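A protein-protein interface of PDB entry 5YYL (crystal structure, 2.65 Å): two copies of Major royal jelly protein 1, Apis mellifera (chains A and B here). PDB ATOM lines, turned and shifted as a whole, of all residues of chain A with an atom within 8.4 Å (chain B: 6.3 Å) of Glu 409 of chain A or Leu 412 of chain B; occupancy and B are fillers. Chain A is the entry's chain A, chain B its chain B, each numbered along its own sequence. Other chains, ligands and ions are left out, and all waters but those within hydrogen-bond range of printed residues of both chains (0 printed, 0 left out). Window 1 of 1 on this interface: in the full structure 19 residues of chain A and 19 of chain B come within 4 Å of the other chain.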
ATOM      1  N   GLU A  25     -37.332  13.038  16.835  1.00  0.00           N
ATOM      2  CA  GLU A  25     -36.478  14.157  17.260  1.00  0.00           C
ATOM      3  C   GLU A  25     -35.676  14.823  16.086  1.00  0.00           C
ATOM      4  O   GLU A  25     -34.620  15.425  16.323  1.00  0.00           O
ATOM      5  CB  GLU A  25     -35.566  13.701  18.449  1.00  0.00           C
ATOM      6  CG  GLU A  25     -36.319  13.172  19.698  1.00  0.00           C
ATOM      7  CD  GLU A  25     -35.524  12.193  20.602  1.00  0.00           C
ATOM      8  OE1 GLU A  25     -35.081  12.572  21.717  1.00  0.00           O
ATOM      9  OE2 GLU A  25     -35.365  11.012  20.226  1.00  0.00           O
ATOM     10  N   LYS A  29     -35.007  18.682   9.897  1.00  0.00           N
ATOM     11  CA  LYS A  29     -33.528  18.854  10.045  1.00  0.00           C
ATOM     12  C   LYS A  29     -32.844  18.716   8.693  1.00  0.00           C
ATOM     13  O   LYS A  29     -32.951  17.679   8.072  1.00  0.00           O
ATOM     14  CB  LYS A  29     -32.892  17.871  11.026  1.00  0.00           C
ATOM     15  CG  LYS A  29     -31.374  17.692  10.838  1.00  0.00           C
ATOM     16  CD  LYS A  29     -30.701  17.054  12.045  1.00  0.00           C
ATOM     17  CE  LYS A  29     -29.416  16.309  11.678  1.00  0.00           C
ATOM     18  NZ  LYS A  29     -28.635  15.822  12.865  1.00  0.00           N
ATOM     19  N   PRO A  32     -26.357  21.105   5.774  1.00  0.00           N
ATOM     20  CA  PRO A  32     -25.768  22.261   5.112  1.00  0.00           C
ATOM     21  C   PRO A  32     -25.469  22.074   3.614  1.00  0.00           C
ATOM     22  O   PRO A  32     -24.862  21.090   3.180  1.00  0.00           O
ATOM     23  CB  PRO A  32     -24.450  22.483   5.867  1.00  0.00           C
ATOM     24  CG  PRO A  32     -24.211  21.254   6.624  1.00  0.00           C
ATOM     25  CD  PRO A  32     -25.565  20.703   6.947  1.00  0.00           C
ATOM     26  N   PHE A 318     -26.684   4.397   4.795  1.00  0.00           N
ATOM     27  CA  PHE A 318     -27.603   5.505   4.614  1.00  0.00           C
ATOM     28  C   PHE A 318     -28.411   5.271   3.357  1.00  0.00           C
ATOM     29  O   PHE A 318     -27.922   4.660   2.402  1.00  0.00           O
ATOM     30  CB  PHE A 318     -26.854   6.818   4.503  1.00  0.00           C
ATOM     31  CG  PHE A 318     -26.242   7.262   5.788  1.00  0.00           C
ATOM     32  CD1 PHE A 318     -26.939   8.105   6.638  1.00  0.00           C
ATOM     33  CD2 PHE A 318     -24.971   6.834   6.148  1.00  0.00           C
ATOM     34  CE1 PHE A 318     -26.386   8.511   7.837  1.00  0.00           C
ATOM     35  CE2 PHE A 318     -24.409   7.236   7.344  1.00  0.00           C
ATOM     36  CZ  PHE A 318     -25.120   8.073   8.194  1.00  0.00           C
ATOM     37  N   VAL A 344     -32.748  10.139   9.866  1.00  0.00           N
ATOM     38  CA  VAL A 344     -31.745  11.008  10.463  1.00  0.00           C
ATOM     39  C   VAL A 344     -31.814  12.469   9.995  1.00  0.00           C
ATOM     40  O   VAL A 344     -31.326  13.341  10.679  1.00  0.00           O
ATOM     41  CB  VAL A 344     -30.357  10.392  10.182  1.00  0.00           C
ATOM     42  CG1 VAL A 344     -29.820  10.764   8.797  1.00  0.00           C
ATOM     43  CG2 VAL A 344     -29.384  10.760  11.263  1.00  0.00           C
ATOM     44  N   ASN A 374     -13.522  12.854  13.907  1.00  0.00           N
ATOM     45  CA  ASN A 374     -14.587  12.160  13.194  1.00  0.00           C
ATOM     46  C   ASN A 374     -14.383  12.444  11.730  1.00  0.00           C
ATOM     47  O   ASN A 374     -14.804  13.494  11.252  1.00  0.00           O
ATOM     48  CB  ASN A 374     -15.956  12.656  13.644  1.00  0.00           C
ATOM     49  CG  ASN A 374     -16.302  12.207  15.037  1.00  0.00           C
ATOM     50  OD1 ASN A 374     -15.905  11.125  15.465  1.00  0.00           O
ATOM     51  ND2 ASN A 374     -17.035  13.032  15.756  1.00  0.00           N
ATOM     52  N   GLU A 376     -15.205  10.906   8.710  1.00  0.00           N
ATOM     53  CA  GLU A 376     -16.132  10.602   7.618  1.00  0.00           C
ATOM     54  C   GLU A 376     -17.236  11.632   7.498  1.00  0.00           C
ATOM     55  O   GLU A 376     -17.828  12.023   8.501  1.00  0.00           O
ATOM     56  CB  GLU A 376     -16.799   9.241   7.815  1.00  0.00           C
ATOM     57  CG  GLU A 376     -15.957   8.066   7.361  1.00  0.00           C
ATOM     58  CD  GLU A 376     -16.666   6.735   7.593  1.00  0.00           C
ATOM     59  OE1 GLU A 376     -16.694   5.924   6.606  1.00  0.00           O
ATOM     60  OE2 GLU A 376     -17.193   6.505   8.732  1.00  0.00           O
ATOM     61  N   TYR A 377     -17.514  12.037   6.260  1.00  0.00           N
ATOM     62  CA  TYR A 377     -18.621  12.934   5.930  1.00  0.00           C
ATOM     63  C   TYR A 377     -19.348  12.471   4.682  1.00  0.00           C
ATOM     64  O   TYR A 377     -18.773  11.792   3.828  1.00  0.00           O
ATOM     65  CB  TYR A 377     -18.126  14.376   5.734  1.00  0.00           C
ATOM     66  CG  TYR A 377     -17.101  14.589   4.643  1.00  0.00           C
ATOM     67  CD1 TYR A 377     -15.744  14.376   4.872  1.00  0.00           C
ATOM     68  CD2 TYR A 377     -17.484  15.055   3.384  1.00  0.00           C
ATOM     69  CE1 TYR A 377     -14.813  14.592   3.864  1.00  0.00           C
ATOM     70  CE2 TYR A 377     -16.547  15.287   2.368  1.00  0.00           C
ATOM     71  CZ  TYR A 377     -15.225  15.047   2.605  1.00  0.00           C
ATOM     72  OH  TYR A 377     -14.307  15.254   1.600  1.00  0.00           O
ATOM     73  N   ALA A 405     -22.594  16.651   5.414  1.00  0.00           N
ATOM     74  CA  ALA A 405     -22.646  16.562   6.873  1.00  0.00           C
ATOM     75  C   ALA A 405     -21.622  15.571   7.368  1.00  0.00           C
ATOM     76  O   ALA A 405     -21.191  14.673   6.630  1.00  0.00           O
ATOM     77  CB  ALA A 405     -24.017  16.139   7.334  1.00  0.00           C
ATOM     78  N   ASN A 406     -21.234  15.736   8.629  1.00  0.00           N
ATOM     79  CA  ASN A 406     -20.363  14.774   9.293  1.00  0.00           C
ATOM     80  C   ASN A 406     -21.194  13.561   9.647  1.00  0.00           C
ATOM     81  O   ASN A 406     -22.291  13.704  10.182  1.00  0.00           O
ATOM     82  CB  ASN A 406     -19.766  15.359  10.565  1.00  0.00           C
ATOM     83  CG  ASN A 406     -18.841  14.396  11.255  1.00  0.00           C
ATOM     84  OD1 ASN A 406     -19.185  13.802  12.259  1.00  0.00           O
ATOM     85  ND2 ASN A 406     -17.666  14.211  10.692  1.00  0.00           N
ATOM     86  N   VAL A 407     -20.663  12.378   9.356  1.00  0.00           N
ATOM     87  CA  VAL A 407     -21.403  11.139   9.542  1.00  0.00           C
ATOM     88  C   VAL A 407     -21.709  10.934  11.021  1.00  0.00           C
ATOM     89  O   VAL A 407     -22.874  10.710  11.378  1.00  0.00           O
ATOM     90  CB  VAL A 407     -20.646   9.925   8.970  1.00  0.00           C
ATOM     91  CG1 VAL A 407     -21.210   8.607   9.494  1.00  0.00           C
ATOM     92  CG2 VAL A 407     -20.712   9.944   7.461  1.00  0.00           C
ATOM     93  N   ASN A 408     -20.671  11.030  11.856  1.00  0.00           N
ATOM     94  CA  ASN A 408     -20.789  10.751  13.280  1.00  0.00           C
ATOM     95  C   ASN A 408     -21.762  11.726  13.948  1.00  0.00           C
ATOM     96  O   ASN A 408     -22.603  11.294  14.727  1.00  0.00           O
ATOM     97  CB  ASN A 408     -19.411  10.783  13.956  1.00  0.00           C
ATOM     98  CG  ASN A 408     -19.463  10.424  15.428  1.00  0.00           C
ATOM     99  OD1 ASN A 408     -19.808  11.262  16.262  1.00  0.00           O
ATOM    100  N   GLU A 409     -21.669  13.014  13.625  1.00  0.00           N
ATOM    101  CA  GLU A 409     -22.619  14.028  14.127  1.00  0.00           C
ATOM    102  C   GLU A 409     -24.094  13.739  13.748  1.00  0.00           C
ATOM    103  O   GLU A 409     -25.019  14.111  14.467  1.00  0.00           O
ATOM    104  CB  GLU A 409     -22.215  15.435  13.647  1.00  0.00           C
ATOM    105  CG  GLU A 409     -22.652  16.581  14.559  1.00  0.00           C
ATOM    106  CD  GLU A 409     -22.014  17.953  14.238  1.00  0.00           C
ATOM    107  OE1 GLU A 409     -22.707  18.990  14.433  1.00  0.00           O
ATOM    108  OE2 GLU A 409     -20.829  18.026  13.820  1.00  0.00           O
ATOM    109  N   LEU A 410     -24.312  13.074  12.620  1.00  0.00           N
ATOM    110  CA  LEU A 410     -25.658  12.820  12.099  1.00  0.00           C
ATOM    111  C   LEU A 410     -26.336  11.697  12.891  1.00  0.00           C
ATOM    112  O   LEU A 410     -27.522  11.770  13.184  1.00  0.00           O
ATOM    113  CB  LEU A 410     -25.544  12.478  10.599  1.00  0.00           C
ATOM    114  CG  LEU A 410     -26.659  12.634   9.562  1.00  0.00           C
ATOM    115  CD1 LEU A 410     -27.421  13.934   9.694  1.00  0.00           C
ATOM    116  CD2 LEU A 410     -26.070  12.518   8.168  1.00  0.00           C
ATOM    117  N   ILE A 411     -25.564  10.691  13.271  1.00  0.00           N
ATOM    118  CA  ILE A 411     -26.071   9.488  13.921  1.00  0.00           C
ATOM    119  C   ILE A 411     -25.830   9.407  15.444  1.00  0.00           C
ATOM    120  O   ILE A 411     -26.374   8.518  16.091  1.00  0.00           O
ATOM    121  CB  ILE A 411     -25.490   8.209  13.277  1.00  0.00           C
ATOM    122  CG1 ILE A 411     -23.974   8.081  13.544  1.00  0.00           C
ATOM    123  CG2 ILE A 411     -25.810   8.183  11.799  1.00  0.00           C
ATOM    124  CD1 ILE A 411     -23.289   6.976  12.763  1.00  0.00           C
ATOM    125  N   LEU A 412     -25.045  10.329  16.005  1.00  0.00           N
ATOM    126  CA  LEU A 412     -24.698  10.327  17.431  1.00  0.00           C
ATOM    127  C   LEU A 412     -25.941  10.307  18.299  1.00  0.00           C
ATOM    128  O   LEU A 412     -26.878  11.053  18.038  1.00  0.00           O
ATOM    129  CB  LEU A 412     -23.881  11.584  17.799  1.00  0.00           C
ATOM    130  CG  LEU A 412     -23.306  11.649  19.228  1.00  0.00           C
ATOM    131  CD1 LEU A 412     -22.257  10.568  19.448  1.00  0.00           C
ATOM    132  CD2 LEU A 412     -22.720  13.028  19.465  1.00  0.00           C
ATOM    133  N   ASN A 413     -25.919   9.480  19.347  1.00  0.00           N
ATOM    134  CA  ASN A 413     -27.076   9.259  20.230  1.00  0.00           C
ATOM    135  C   ASN A 413     -28.335   8.778  19.462  1.00  0.00           C
ATOM    136  O   ASN A 413     -29.460   9.234  19.748  1.00  0.00           O
ATOM    137  CB  ASN A 413     -27.415  10.537  21.039  1.00  0.00           C
ATOM    138  CG  ASN A 413     -26.210  11.139  21.747  1.00  0.00           C
ATOM    139  OD1 ASN A 413     -25.320  10.431  22.177  1.00  0.00           O
ATOM    140  ND2 ASN A 413     -26.193  12.461  21.880  1.00  0.00           N
ATOM    141  N   THR A 414     -28.138   7.916  18.464  1.00  0.00           N
ATOM    142  CA  THR A 414     -29.248   7.272  17.746  1.00  0.00           C
ATOM    143  C   THR A 414     -28.892   5.815  17.548  1.00  0.00           C
ATOM    144  O   THR A 414     -27.723   5.449  17.670  1.00  0.00           O
ATOM    145  CB  THR A 414     -29.569   7.900  16.350  1.00  0.00           C
ATOM    146  OG1 THR A 414     -28.621   7.464  15.370  1.00  0.00           O
ATOM    147  CG2 THR A 414     -29.584   9.434  16.397  1.00  0.00           C
ATOM    148  N   GLU A 417     -25.678   4.737  15.580  1.00  0.00           N
ATOM    149  CA  GLU A 417     -24.288   5.062  15.956  1.00  0.00           C
ATOM    150  C   GLU A 417     -23.426   3.839  16.214  1.00  0.00           C
ATOM    151  O   GLU A 417     -23.932   2.769  16.550  1.00  0.00           O
ATOM    152  CB  GLU A 417     -24.212   5.994  17.167  1.00  0.00           C
ATOM    153  CG  GLU A 417     -24.462   5.388  18.532  1.00  0.00           C
ATOM    154  CD  GLU A 417     -24.291   6.419  19.652  1.00  0.00           C
ATOM    155  OE1 GLU A 417     -23.214   7.071  19.733  1.00  0.00           O
ATOM    156  OE2 GLU A 417     -25.219   6.574  20.472  1.00  0.00           O
ATOM    157  N   LYS A 427     -12.612  16.399  20.351  1.00  0.00           N
ATOM    158  CA  LYS A 427     -12.998  15.631  19.167  1.00  0.00           C
ATOM    159  C   LYS A 427     -13.419  16.620  18.100  1.00  0.00           C
ATOM    160  O   LYS A 427     -14.245  17.496  18.376  1.00  0.00           O
ATOM    161  CB  LYS A 427     -14.153  14.674  19.477  1.00  0.00           C
ATOM    162  CG  LYS A 427     -14.258  13.484  18.535  1.00  0.00           C
ATOM    163  CD  LYS A 427     -13.066  12.538  18.710  1.00  0.00           C
ATOM    164  CE  LYS A 427     -13.472  11.075  18.712  1.00  0.00           C
ATOM    165  NZ  LYS A 427     -13.826  10.563  17.351  1.00  0.00           N
ATOM    166  N   ILE A 428     -12.835  16.501  16.906  1.00  0.00           N
ATOM    167  CA  ILE A 428     -13.156  17.394  15.790  1.00  0.00           C
ATOM    168  C   ILE A 428     -14.026  16.717  14.738  1.00  0.00           C
ATOM    169  O   ILE A 428     -13.653  15.691  14.149  1.00  0.00           O
ATOM    170  CB  ILE A 428     -11.896  17.930  15.099  1.00  0.00           C
ATOM    171  CG1 ILE A 428     -10.879  18.358  16.158  1.00  0.00           C
ATOM    172  CG2 ILE A 428     -12.289  19.076  14.157  1.00  0.00           C
ATOM    173  CD1 ILE A 428      -9.790  19.283  15.672  1.00  0.00           C
ATOM    174  N   SER A 429     -15.185  17.315  14.492  1.00  0.00           N
ATOM    175  CA  SER A 429     -16.078  16.847  13.430  1.00  0.00           C
ATOM    176  C   SER A 429     -15.833  17.633  12.135  1.00  0.00           C
ATOM    177  O   SER A 429     -15.743  18.858  12.158  1.00  0.00           O
ATOM    178  CB  SER A 429     -17.525  16.953  13.876  1.00  0.00           C
ATOM    179  OG  SER A 429     -17.804  15.871  14.732  1.00  0.00           O
ATOM    180  N   ILE A 430     -15.711  16.901  11.026  1.00  0.00           N
ATOM    181  CA  ILE A 430     -15.367  17.466   9.735  1.00  0.00           C
ATOM    182  C   ILE A 430     -16.456  17.242   8.696  1.00  0.00           C
ATOM    183  O   ILE A 430     -17.059  16.175   8.640  1.00  0.00           O
ATOM    184  CB  ILE A 430     -14.117  16.782   9.192  1.00  0.00           C
ATOM    185  CG1 ILE A 430     -12.976  16.873  10.192  1.00  0.00           C
ATOM    186  CG2 ILE A 430     -13.706  17.389   7.856  1.00  0.00           C
ATOM    187  CD1 ILE A 430     -12.527  18.289  10.510  1.00  0.00           C
ATOM    188  N   HIS A 431     -16.685  18.272   7.889  1.00  0.00           N
ATOM    189  CA  HIS A 431     -17.200  18.107   6.523  1.00  0.00           C
ATOM    190  C   HIS A 431     -16.637  19.244   5.650  1.00  0.00           C
ATOM    191  O   HIS A 431     -15.723  19.946   6.088  1.00  0.00           O
ATOM    192  CB  HIS A 431     -18.728  18.021   6.510  1.00  0.00           C
ATOM    193  CG  HIS A 431     -19.426  19.200   7.097  1.00  0.00           C
ATOM    194  ND1 HIS A 431     -19.321  20.464   6.566  1.00  0.00           N
ATOM    195  CD2 HIS A 431     -20.279  19.303   8.148  1.00  0.00           C
ATOM    196  CE1 HIS A 431     -20.076  21.296   7.265  1.00  0.00           C
ATOM    197  NE2 HIS A 431     -20.656  20.620   8.238  1.00  0.00           N
ATOM    198  N   ASN B 374     -17.996  23.565  20.521  1.00  0.00           N
ATOM    199  CA  ASN B 374     -18.949  23.196  21.566  1.00  0.00           C
ATOM    200  C   ASN B 374     -18.220  23.398  22.878  1.00  0.00           C
ATOM    201  O   ASN B 374     -17.488  22.513  23.314  1.00  0.00           O
ATOM    202  CB  ASN B 374     -19.389  21.745  21.415  1.00  0.00           C
ATOM    203  CG  ASN B 374     -20.260  21.533  20.205  1.00  0.00           C
ATOM    204  OD1 ASN B 374     -21.021  22.407  19.806  1.00  0.00           O
ATOM    205  ND2 ASN B 374     -20.165  20.357  19.626  1.00  0.00           N
ATOM    206  N   VAL B 407     -21.096  18.845  26.765  1.00  0.00           N
ATOM    207  CA  VAL B 407     -22.540  18.982  26.920  1.00  0.00           C
ATOM    208  C   VAL B 407     -23.255  18.634  25.625  1.00  0.00           C
ATOM    209  O   VAL B 407     -24.191  17.809  25.626  1.00  0.00           O
ATOM    210  CB  VAL B 407     -22.925  20.398  27.408  1.00  0.00           C
ATOM    211  CG1 VAL B 407     -24.400  20.705  27.177  1.00  0.00           C
ATOM    212  CG2 VAL B 407     -22.564  20.545  28.882  1.00  0.00           C
ATOM    213  N   ASN B 408     -22.802  19.249  24.532  1.00  0.00           N
ATOM    214  CA  ASN B 408     -23.452  19.103  23.233  1.00  0.00           C
ATOM    215  C   ASN B 408     -23.402  17.664  22.754  1.00  0.00           C
ATOM    216  O   ASN B 408     -24.413  17.155  22.290  1.00  0.00           O
ATOM    217  CB  ASN B 408     -22.835  20.061  22.209  1.00  0.00           C
ATOM    218  CG  ASN B 408     -23.498  19.990  20.831  1.00  0.00           C
ATOM    219  OD1 ASN B 408     -24.632  19.535  20.652  1.00  0.00           O
ATOM    220  N   GLU B 409     -22.253  16.998  22.900  1.00  0.00           N
ATOM    221  CA  GLU B 409     -22.130  15.554  22.569  1.00  0.00           C
ATOM    222  C   GLU B 409     -23.116  14.649  23.353  1.00  0.00           C
ATOM    223  O   GLU B 409     -23.543  13.605  22.875  1.00  0.00           O
ATOM    224  CB  GLU B 409     -20.681  15.068  22.796  1.00  0.00           C
ATOM    225  CG  GLU B 409     -19.629  15.650  21.858  1.00  0.00           C
ATOM    226  N   LEU B 410     -23.474  15.066  24.556  1.00  0.00           N
ATOM    227  CA  LEU B 410     -24.321  14.269  25.446  1.00  0.00           C
ATOM    228  C   LEU B 410     -25.791  14.305  25.004  1.00  0.00           C
ATOM    229  O   LEU B 410     -26.480  13.302  25.064  1.00  0.00           O
ATOM    230  CB  LEU B 410     -24.141  14.777  26.895  1.00  0.00           C
ATOM    231  CG  LEU B 410     -24.154  13.816  28.081  1.00  0.00           C
ATOM    232  CD1 LEU B 410     -23.173  12.664  27.932  1.00  0.00           C
ATOM    233  CD2 LEU B 410     -23.847  14.626  29.345  1.00  0.00           C
ATOM    234  N   ILE B 411     -26.232  15.456  24.514  1.00  0.00           N
ATOM    235  CA  ILE B 411     -27.638  15.688  24.136  1.00  0.00           C
ATOM    236  C   ILE B 411     -27.934  15.694  22.625  1.00  0.00           C
ATOM    237  O   ILE B 411     -29.117  15.758  22.232  1.00  0.00           O
ATOM    238  CB  ILE B 411     -28.142  17.035  24.721  1.00  0.00           C
ATOM    239  CG1 ILE B 411     -27.424  18.241  24.074  1.00  0.00           C
ATOM    240  CG2 ILE B 411     -27.967  17.045  26.238  1.00  0.00           C
ATOM    241  CD1 ILE B 411     -27.667  19.572  24.750  1.00  0.00           C
ATOM    242  N   LEU B 412     -26.890  15.656  21.786  1.00  0.00           N
ATOM    243  CA  LEU B 412     -27.063  15.848  20.329  1.00  0.00           C
ATOM    244  C   LEU B 412     -28.024  14.817  19.751  1.00  0.00           C
ATOM    245  O   LEU B 412     -27.924  13.641  20.095  1.00  0.00           O
ATOM    246  CB  LEU B 412     -25.723  15.730  19.600  1.00  0.00           C
ATOM    247  CG  LEU B 412     -25.710  16.038  18.102  1.00  0.00           C
ATOM    248  CD1 LEU B 412     -25.985  17.511  17.856  1.00  0.00           C
ATOM    249  CD2 LEU B 412     -24.395  15.626  17.468  1.00  0.00           C
ATOM    250  N   ASN B 413     -28.914  15.258  18.857  1.00  0.00           N
ATOM    251  CA  ASN B 413     -29.960  14.393  18.275  1.00  0.00           C
ATOM    252  C   ASN B 413     -30.879  13.769  19.341  1.00  0.00           C
ATOM    253  O   ASN B 413     -31.272  12.604  19.230  1.00  0.00           O
ATOM    254  CB  ASN B 413     -29.356  13.287  17.375  1.00  0.00           C
ATOM    255  CG  ASN B 413     -28.361  13.822  16.351  1.00  0.00           C
ATOM    256  OD1 ASN B 413     -28.491  14.939  15.854  1.00  0.00           O
ATOM    257  ND2 ASN B 413     -27.370  13.014  16.026  1.00  0.00           N
ATOM    258  N   THR B 414     -31.187  14.539  20.386  1.00  0.00           N
ATOM    259  CA  THR B 414     -32.165  14.131  21.410  1.00  0.00           C
ATOM    260  C   THR B 414     -33.043  15.332  21.704  1.00  0.00           C
ATOM    261  O   THR B 414     -32.684  16.454  21.361  1.00  0.00           O
ATOM    262  CB  THR B 414     -31.516  13.639  22.741  1.00  0.00           C
ATOM    263  OG1 THR B 414     -31.054  14.756  23.532  1.00  0.00           O
ATOM    264  CG2 THR B 414     -30.361  12.665  22.487  1.00  0.00           C
ATOM    265  N   GLU B 417     -31.540  18.707  22.965  1.00  0.00           N
ATOM    266  CA  GLU B 417     -30.564  19.528  22.231  1.00  0.00           C
ATOM    267  C   GLU B 417     -31.036  20.934  21.942  1.00  0.00           C
ATOM    268  O   GLU B 417     -32.242  21.190  21.869  1.00  0.00           O
ATOM    269  CB  GLU B 417     -30.096  18.865  20.932  1.00  0.00           C
ATOM    270  CG  GLU B 417     -31.069  18.936  19.751  1.00  0.00           C
ATOM    271  CD  GLU B 417     -30.484  18.347  18.484  1.00  0.00           C
ATOM    272  OE1 GLU B 417     -29.381  18.779  18.068  1.00  0.00           O
ATOM    273  OE2 GLU B 417     -31.110  17.431  17.913  1.00  0.00           O
ATOM    274  N   ASN B 418     -30.062  21.836  21.806  1.00  0.00           N
ATOM    275  CA  ASN B 418     -30.302  23.170  21.286  1.00  0.00           C
ATOM    276  C   ASN B 418     -30.116  23.117  19.774  1.00  0.00           C
ATOM    277  O   ASN B 418     -29.338  22.296  19.270  1.00  0.00           O
ATOM    278  CB  ASN B 418     -29.359  24.190  21.922  1.00  0.00           C
ATOM    279  N   ASP B 420     -29.050  23.132  16.121  1.00  0.00           N
ATOM    280  CA  ASP B 420     -27.718  23.178  15.507  1.00  0.00           C
ATOM    281  C   ASP B 420     -27.755  23.937  14.183  1.00  0.00           C
ATOM    282  O   ASP B 420     -28.434  23.517  13.245  1.00  0.00           O
ATOM    283  CB  ASP B 420     -27.174  21.763  15.268  1.00  0.00           C
ATOM    284  N   ASP B 422     -25.477  24.281  11.335  1.00  0.00           N
ATOM    285  CA  ASP B 422     -24.341  23.526  10.800  1.00  0.00           C
ATOM    286  C   ASP B 422     -23.684  24.383   9.710  1.00  0.00           C
ATOM    287  O   ASP B 422     -23.867  24.146   8.529  1.00  0.00           O
ATOM    288  CB  ASP B 422     -24.839  22.163  10.282  1.00  0.00           C
ATOM    289  CG  ASP B 422     -23.718  21.147  10.063  1.00  0.00           C
ATOM    290  OD1 ASP B 422     -22.539  21.546   9.920  1.00  0.00           O
ATOM    291  OD2 ASP B 422     -24.032  19.928  10.009  1.00  0.00           O
ATOM    292  N   LYS B 427     -16.330  21.386  13.695  1.00  0.00           N
ATOM    293  CA  LYS B 427     -16.836  21.692  15.035  1.00  0.00           C
ATOM    294  C   LYS B 427     -15.981  20.922  16.017  1.00  0.00           C
ATOM    295  O   LYS B 427     -15.789  19.703  15.848  1.00  0.00           O
ATOM    296  CB  LYS B 427     -18.299  21.263  15.159  1.00  0.00           C
ATOM    297  CG  LYS B 427     -19.063  21.999  16.239  1.00  0.00           C
ATOM    298  CD  LYS B 427     -19.251  23.475  15.911  1.00  0.00           C
ATOM    299  CE  LYS B 427     -20.715  23.937  16.048  1.00  0.00           C
ATOM    300  NZ  LYS B 427     -21.194  24.008  17.464  1.00  0.00           N
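Among the printed residues, merely in contact across the chains: Glu 25 of chain A with Thr 414 of chain B, Pro 32 of chain A with Asp 422 of chain B, Glu 409 of chain A with Leu 412 of chain B, Ile 411 of chain A with Asn 413 of chain B, Leu 412 of chain A with Glu 409 of chain B, Asn 413 of chain A with Ile 411 of chain B, Asn 413 of chain A with Asn 413 of chain B, Asn 413 of chain A with Thr 414 of chain B, Thr 414 of chain A with Asn 413 of chain B, Lys 427 of chain A with Lys 427 of chain B and Ile 428 of chain A with Lys 427 of chain B.
O of Ile 411 of chain A lies within hydrogen-bond range of OG1 of Thr 414 of chain A (2.6 Å).
The backbone carbonyl oxygen of Ile 411 of chain B sits at hydrogen-bond distance from the side-chain hydroxyl of Thr 414 of chain B (2.5 Å).
The side-chain carboxylate (OE2) of Glu 417 of chain B sits at hydrogen-bond distance from the backbone NH (N) of Asn 413 of chain B.
Glu 409 of chain A touches Asn 413 of chain B, and with the chains exchanged Asn 413 of chain A touches Glu 409 of chain B.
Leu 410 of chain A touches Asn 413 of chain B, and with the chains exchanged Asn 413 of chain A touches Leu 410 of chain B.
Leu 412 of chain B touches its own counterpart, Leu 412 of chain A.
Asn 413 of chain A touches its own counterpart, Asn 413 of chain B.
Of the printed residues of chain B, Glu 25 of chain A touches Thr 414.
Of the printed residues of chain B, Glu 409 of chain A touches Leu 412 and Asn 413.
Printed residues of chain B within 4 Å of Ile 428 of chain A: Lys 427.
Of the printed residues of chain B, His 431 of chain A touches Asp 422 (2.7 Å).
Of chain A, only Glu 409 (3.4 Å), Leu 412 (3.5 Å) and Asn 413 (2.8 Å) come within 4 Å of Leu 412 of chain B.
The nearest residue of chain B that does not touch Glu 409 of chain A is Lys 427 of chain B (4.3 Å).
The nearest printed residue of chain A that does not touch Leu 410 of chain B is Leu 412 of chain A (5.5 Å).
NZ of Lys 29 of chain A lies within hydrogen-bond range of OD1 of Asn 413 of chain B (3.1 Å).
The side-chain amide nitrogen of Asn 413 of chain B lies within hydrogen-bond range of the backbone carbonyl oxygen of Glu 409 of chain A (3.0 Å).
O of Leu 410 of chain A is in hydrogen-bond range of ND2 of Asn 413 of chain B (3.1 Å).
The side-chain amide nitrogen of Asn 413 of chain B lies within hydrogen-bond range of the backbone carbonyl oxygen of Leu 412 of chain A.
The side-chain amide nitrogen of Asn 413 of chain A is in hydrogen-bond range of the backbone carbonyl oxygen of Glu 409 of chain B, 3.1 Å away.
ND2 of Asn 413 of chain A sits at hydrogen-bond distance from O of Leu 410 of chain B, at 3.3 Å.
ND2 of Asn 413 of chain A lies within hydrogen-bond range of O of Leu 412 of chain B, 2.8 Å away.
The backbone NH (N) of Ser 429 of chain A is in hydrogen-bond range of the backbone carbonyl oxygen (O) of Lys 427 of chain B, at 2.8 Å.
A ring nitrogen (NE2) of His 431 of chain A is in hydrogen-bond range of the side-chain carboxylate (OD1) of Asp 422 of chain B (2.7 Å).
The backbone carbonyl oxygen of Leu 412 of chain A lies close to the backbone carbonyl oxygen of Leu 412 of chain B (3.5 Å).
Printed residues of chain A that touch a printed residue of chain B: Glu 25, Lys 29, Pro 32, Glu 409, Leu 410, Ile 411, Leu 412, Asn 413, Thr 414, Lys 427, Ile 428, Ser 429 and His 431.
Printed residues of chain B that touch a printed residue of chain A: Glu 409, Leu 410, Ile 411, Leu 412, Asn 413, Thr 414, Asp 422 and Lys 427.
Hydrophobic or aromatic side chains of chain B within 4 Å of the printed part of chain A: Leu 412.
Among the printed residues, no Asp or Glu carboxylate lies within 4 Å of a Lys or Arg side-chain nitrogen of the other chain.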
